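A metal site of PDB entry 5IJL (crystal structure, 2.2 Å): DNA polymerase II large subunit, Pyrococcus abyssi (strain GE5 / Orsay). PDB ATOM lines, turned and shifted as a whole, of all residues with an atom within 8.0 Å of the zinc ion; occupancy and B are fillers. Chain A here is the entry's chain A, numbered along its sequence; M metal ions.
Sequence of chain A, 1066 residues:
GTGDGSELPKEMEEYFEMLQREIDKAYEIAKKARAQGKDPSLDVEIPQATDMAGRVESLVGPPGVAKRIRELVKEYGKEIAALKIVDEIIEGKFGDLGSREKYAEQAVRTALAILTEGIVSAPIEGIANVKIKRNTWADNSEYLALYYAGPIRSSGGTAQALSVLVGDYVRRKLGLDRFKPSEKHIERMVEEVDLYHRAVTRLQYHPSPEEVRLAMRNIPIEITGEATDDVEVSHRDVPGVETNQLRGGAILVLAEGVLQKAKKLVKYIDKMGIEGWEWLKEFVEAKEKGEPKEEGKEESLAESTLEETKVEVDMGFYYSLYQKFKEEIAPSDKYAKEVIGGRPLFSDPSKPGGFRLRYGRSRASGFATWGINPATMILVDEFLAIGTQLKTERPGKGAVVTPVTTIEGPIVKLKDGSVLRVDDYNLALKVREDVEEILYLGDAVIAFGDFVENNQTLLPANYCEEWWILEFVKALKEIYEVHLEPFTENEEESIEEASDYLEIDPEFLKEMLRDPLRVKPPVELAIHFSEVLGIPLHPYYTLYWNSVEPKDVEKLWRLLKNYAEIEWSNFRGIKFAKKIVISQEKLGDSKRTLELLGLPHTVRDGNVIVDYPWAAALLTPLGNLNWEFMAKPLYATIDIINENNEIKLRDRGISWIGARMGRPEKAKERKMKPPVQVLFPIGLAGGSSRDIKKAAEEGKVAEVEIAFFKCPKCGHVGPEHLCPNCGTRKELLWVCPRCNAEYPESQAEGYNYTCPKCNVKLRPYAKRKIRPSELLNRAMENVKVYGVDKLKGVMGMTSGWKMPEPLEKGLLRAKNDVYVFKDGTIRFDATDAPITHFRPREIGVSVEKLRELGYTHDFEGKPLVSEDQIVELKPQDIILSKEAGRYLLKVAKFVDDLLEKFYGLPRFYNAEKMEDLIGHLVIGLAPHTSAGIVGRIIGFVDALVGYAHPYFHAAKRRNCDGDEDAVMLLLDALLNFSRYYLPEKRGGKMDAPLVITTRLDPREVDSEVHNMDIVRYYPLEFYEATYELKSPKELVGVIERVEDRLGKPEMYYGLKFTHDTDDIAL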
ATOM      1  N   VAL A 735     -12.449  13.519  11.549  1.00  0.00           N
ATOM      2  CA  VAL A 735     -11.906  12.278  10.991  1.00  0.00           C
ATOM      3  C   VAL A 735     -10.374  12.295  10.966  1.00  0.00           C
ATOM      4  O   VAL A 735      -9.785  13.332  10.658  1.00  0.00           O
ATOM      5  CB  VAL A 735     -12.506  12.020   9.582  1.00  0.00           C
ATOM      6  CG1 VAL A 735     -12.016  10.702   8.985  1.00  0.00           C
ATOM      7  CG2 VAL A 735     -14.041  12.040   9.616  1.00  0.00           C
ATOM      8  N   CYS A 736      -9.731  11.147  11.260  1.00  0.00           N
ATOM      9  CA  CYS A 736      -8.276  11.036  11.104  1.00  0.00           C
ATOM     10  C   CYS A 736      -8.034  10.683   9.624  1.00  0.00           C
ATOM     11  O   CYS A 736      -8.641   9.722   9.138  1.00  0.00           O
ATOM     12  CB  CYS A 736      -7.668   9.992  12.042  1.00  0.00           C
ATOM     13  SG  CYS A 736      -5.903   9.664  11.721  1.00  0.00           S
ATOM     14  N   PRO A 737      -7.188  11.447   8.898  1.00  0.00           N
ATOM     15  CA  PRO A 737      -6.971  11.114   7.474  1.00  0.00           C
ATOM     16  C   PRO A 737      -6.219   9.795   7.226  1.00  0.00           C
ATOM     17  O   PRO A 737      -6.143   9.367   6.072  1.00  0.00           O
ATOM     18  CB  PRO A 737      -6.247  12.347   6.929  1.00  0.00           C
ATOM     19  CG  PRO A 737      -5.607  12.978   8.103  1.00  0.00           C
ATOM     20  CD  PRO A 737      -6.403  12.629   9.312  1.00  0.00           C
ATOM     21  N   ARG A 738      -5.689   9.118   8.286  1.00  0.00           N
ATOM     22  CA  ARG A 738      -4.976   7.841   8.151  1.00  0.00           C
ATOM     23  C   ARG A 738      -5.837   6.605   8.445  1.00  0.00           C
ATOM     24  O   ARG A 738      -6.057   5.790   7.554  1.00  0.00           O
ATOM     25  CB  ARG A 738      -3.678   7.834   8.990  1.00  0.00           C
ATOM     26  CG  ARG A 738      -2.803   6.612   8.698  1.00  0.00           C
ATOM     27  CD  ARG A 738      -1.550   6.543   9.557  1.00  0.00           C
ATOM     28  NE  ARG A 738      -0.518   7.470   9.090  1.00  0.00           N
ATOM     29  CZ  ARG A 738      -0.058   8.493   9.807  1.00  0.00           C
ATOM     30  NH1 ARG A 738      -0.518   8.709  11.033  1.00  0.00           N
ATOM     31  NH2 ARG A 738       0.886   9.285   9.306  1.00  0.00           N
ATOM     32  N   CYS A 739      -6.284   6.458   9.712  1.00  0.00           N
ATOM     33  CA  CYS A 739      -7.064   5.298  10.170  1.00  0.00           C
ATOM     34  C   CYS A 739      -8.572   5.432   9.936  1.00  0.00           C
ATOM     35  O   CYS A 739      -9.305   4.480  10.221  1.00  0.00           O
ATOM     36  CB  CYS A 739      -6.745   4.985  11.631  1.00  0.00           C
ATOM     37  SG  CYS A 739      -7.065   6.346  12.778  1.00  0.00           S
ATOM     38  N   ASN A 740      -9.016   6.602   9.446  1.00  0.00           N
ATOM     39  CA  ASN A 740     -10.421   6.945   9.187  1.00  0.00           C
ATOM     40  C   ASN A 740     -11.321   6.791  10.433  1.00  0.00           C
ATOM     41  O   ASN A 740     -12.518   6.506  10.319  1.00  0.00           O
ATOM     42  CB  ASN A 740     -10.979   6.187   7.963  1.00  0.00           C
ATOM     43  CG  ASN A 740     -10.574   6.815   6.652  1.00  0.00           C
ATOM     44  OD1 ASN A 740     -10.975   7.951   6.321  1.00  0.00           O
ATOM     45  ND2 ASN A 740      -9.803   6.079   5.868  1.00  0.00           N
ATOM     46  N   ALA A 741     -10.732   6.977  11.621  1.00  0.00           N
ATOM     47  CA  ALA A 741     -11.460   6.935  12.887  1.00  0.00           C
ATOM     48  C   ALA A 741     -12.258   8.249  13.008  1.00  0.00           C
ATOM     49  O   ALA A 741     -11.765   9.301  12.590  1.00  0.00           O
ATOM     50  CB  ALA A 741     -10.492   6.804  14.053  1.00  0.00           C
ATOM     51  N   TYR A 743     -14.317  10.984  15.432  1.00  0.00           N
ATOM     52  CA  TYR A 743     -14.367  11.542  16.775  1.00  0.00           C
ATOM     53  C   TYR A 743     -15.309  12.741  16.838  1.00  0.00           C
ATOM     54  O   TYR A 743     -15.012  13.760  16.211  1.00  0.00           O
ATOM     55  CB  TYR A 743     -12.958  11.973  17.257  1.00  0.00           C
ATOM     56  CG  TYR A 743     -11.919  10.890  17.206  1.00  0.00           C
ATOM     57  CD1 TYR A 743     -11.821   9.937  18.222  1.00  0.00           C
ATOM     58  CD2 TYR A 743     -11.025  10.804  16.150  1.00  0.00           C
ATOM     59  CE1 TYR A 743     -10.868   8.921  18.173  1.00  0.00           C
ATOM     60  CE2 TYR A 743     -10.071   9.790  16.086  1.00  0.00           C
ATOM     61  CZ  TYR A 743     -10.008   8.847  17.093  1.00  0.00           C
ATOM     62  OH  TYR A 743      -9.068   7.843  17.029  1.00  0.00           O
ATOM     63  N   THR A 754      -6.033  16.089  17.202  1.00  0.00           N
ATOM     64  CA  THR A 754      -4.969  15.176  16.766  1.00  0.00           C
ATOM     65  C   THR A 754      -5.432  13.777  17.136  1.00  0.00           C
ATOM     66  O   THR A 754      -5.937  13.584  18.237  1.00  0.00           O
ATOM     67  CB  THR A 754      -3.617  15.523  17.407  1.00  0.00           C
ATOM     68  OG1 THR A 754      -3.442  16.945  17.463  1.00  0.00           O
ATOM     69  CG2 THR A 754      -2.448  14.887  16.665  1.00  0.00           C
ATOM     70  N   CYS A 755      -5.310  12.819  16.208  1.00  0.00           N
ATOM     71  CA  CYS A 755      -5.716  11.429  16.442  1.00  0.00           C
ATOM     72  C   CYS A 755      -4.962  10.839  17.676  1.00  0.00           C
ATOM     73  O   CYS A 755      -3.746  11.020  17.763  1.00  0.00           O
ATOM     74  CB  CYS A 755      -5.497  10.589  15.191  1.00  0.00           C
ATOM     75  SG  CYS A 755      -5.953   8.846  15.361  1.00  0.00           S
ATOM     76  N   PRO A 756      -5.648  10.198  18.656  1.00  0.00           N
ATOM     77  CA  PRO A 756      -4.935   9.656  19.831  1.00  0.00           C
ATOM     78  C   PRO A 756      -3.890   8.560  19.530  1.00  0.00           C
ATOM     79  O   PRO A 756      -2.931   8.452  20.298  1.00  0.00           O
ATOM     80  CB  PRO A 756      -6.051   9.145  20.738  1.00  0.00           C
ATOM     81  CG  PRO A 756      -7.197   8.892  19.826  1.00  0.00           C
ATOM     82  CD  PRO A 756      -7.106   9.935  18.758  1.00  0.00           C
ATOM     83  N   LYS A 757      -4.054   7.785  18.434  1.00  0.00           N
ATOM     84  CA  LYS A 757      -3.082   6.732  18.092  1.00  0.00           C
ATOM     85  C   LYS A 757      -2.447   6.881  16.682  1.00  0.00           C
ATOM     86  O   LYS A 757      -1.967   5.889  16.119  1.00  0.00           O
ATOM     87  CB  LYS A 757      -3.663   5.326  18.320  1.00  0.00           C
ATOM     88  CG  LYS A 757      -3.559   4.893  19.793  1.00  0.00           C
ATOM     89  CD  LYS A 757      -3.182   3.416  19.978  1.00  0.00           C
ATOM     90  CE  LYS A 757      -1.732   3.213  20.343  1.00  0.00           C
ATOM     91  NZ  LYS A 757      -1.415   1.775  20.553  1.00  0.00           N
ATOM     92  N   CYS A 758      -2.380   8.125  16.166  1.00  0.00           N
ATOM     93  CA  CYS A 758      -1.730   8.574  14.919  1.00  0.00           C
ATOM     94  C   CYS A 758      -1.305  10.000  15.246  1.00  0.00           C
ATOM     95  O   CYS A 758      -2.171  10.789  15.638  1.00  0.00           O
ATOM     96  CB  CYS A 758      -2.688   8.560  13.730  1.00  0.00           C
ATOM     97  SG  CYS A 758      -3.161   6.906  13.148  1.00  0.00           S
ATOM     98  N   ASN A 759      -0.036  10.379  15.060  1.00  0.00           N
ATOM     99  CA  ASN A 759       0.352  11.755  15.400  1.00  0.00           C
ATOM    100  C   ASN A 759      -0.114  12.829  14.359  1.00  0.00           C
ATOM    101  O   ASN A 759       0.348  13.977  14.400  1.00  0.00           O
ATOM    102  CB  ASN A 759       1.866  11.862  15.680  1.00  0.00           C
ATOM    103  CG  ASN A 759       2.206  12.932  16.693  1.00  0.00           C
ATOM    104  OD1 ASN A 759       1.460  13.184  17.655  1.00  0.00           O
ATOM    105  ND2 ASN A 759       3.325  13.604  16.482  1.00  0.00           N
ATOM    106  N   VAL A 760      -1.103  12.472  13.493  1.00  0.00           N
ATOM    107  CA  VAL A 760      -1.651  13.375  12.467  1.00  0.00           C
ATOM    108  C   VAL A 760      -2.928  14.093  12.924  1.00  0.00           C
ATOM    109  O   VAL A 760      -3.751  13.517  13.637  1.00  0.00           O
ATOM    110  CB  VAL A 760      -1.860  12.721  11.068  1.00  0.00           C
ATOM    111  CG1 VAL A 760      -0.522  12.517  10.345  1.00  0.00           C
ATOM    112  CG2 VAL A 760      -2.651  11.425  11.152  1.00  0.00           C
ATOM    113  N   LYS A 761      -3.067  15.353  12.473  1.00  0.00           N
ATOM    114  CA  LYS A 761      -4.181  16.246  12.767  1.00  0.00           C
ATOM    115  C   LYS A 761      -5.496  15.754  12.142  1.00  0.00           C
ATOM    116  O   LYS A 761      -5.512  15.241  11.022  1.00  0.00           O
ATOM    117  CB  LYS A 761      -3.876  17.676  12.304  1.00  0.00           C
ATOM    118  CG  LYS A 761      -2.613  18.300  12.903  1.00  0.00           C
ATOM    119  CD  LYS A 761      -2.862  19.006  14.242  1.00  0.00           C
ATOM    120  CE  LYS A 761      -1.661  19.792  14.718  1.00  0.00           C
ATOM    121  NZ  LYS A 761      -1.429  21.034  13.927  1.00  0.00           N
ATOM    122  N   LEU A 762      -6.582  15.894  12.902  1.00  0.00           N
ATOM    123  CA  LEU A 762      -7.941  15.538  12.502  1.00  0.00           C
ATOM    124  C   LEU A 762      -8.496  16.572  11.513  1.00  0.00           C
ATOM    125  O   LEU A 762      -8.091  17.746  11.521  1.00  0.00           O
ATOM    126  CB  LEU A 762      -8.871  15.442  13.742  1.00  0.00           C
ATOM    127  CG  LEU A 762      -8.531  14.383  14.813  1.00  0.00           C
ATOM    128  CD1 LEU A 762      -9.421  14.540  16.060  1.00  0.00           C
ATOM    129  CD2 LEU A 762      -8.641  12.960  14.272  1.00  0.00           C
HETATM  130 ZN    ZN M   1      -5.451   7.915  13.172  1.00  0.00          ZN
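The zinc ion is bound by the side-chain sulfur of Cys 739 (2.3 Å), the side-chain sulfur of Cys 736 (2.3 Å), the side-chain sulfur of Cys 755 (2.4 Å) and the side-chain sulfur of Cys 758 (2.5 Å).
Of the 17 residues printed, 4 come within 4 Å of the zinc ion.
The nearest printed residue that does not touch the zinc ion is Arg 738 (4.5 Å).
The backbone NH of Arg 738 sits close to the side-chain sulfur of Cys 736, 3.5 Å away.
The side-chain sulfur (SG) of Cys 755 sits close to the side-chain hydroxyl (OH) of Tyr 743 (3.7 Å).
The backbone NH (N) of Lys 757 sits close to the side-chain sulfur (SG) of Cys 755 (3.8 Å).
N of Cys 736 sits at hydrogen-bond distance from O of Ala 741.
The backbone NH of Cys 755 sits at hydrogen-bond distance from the backbone carbonyl oxygen of Val 760 (3.1 Å).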
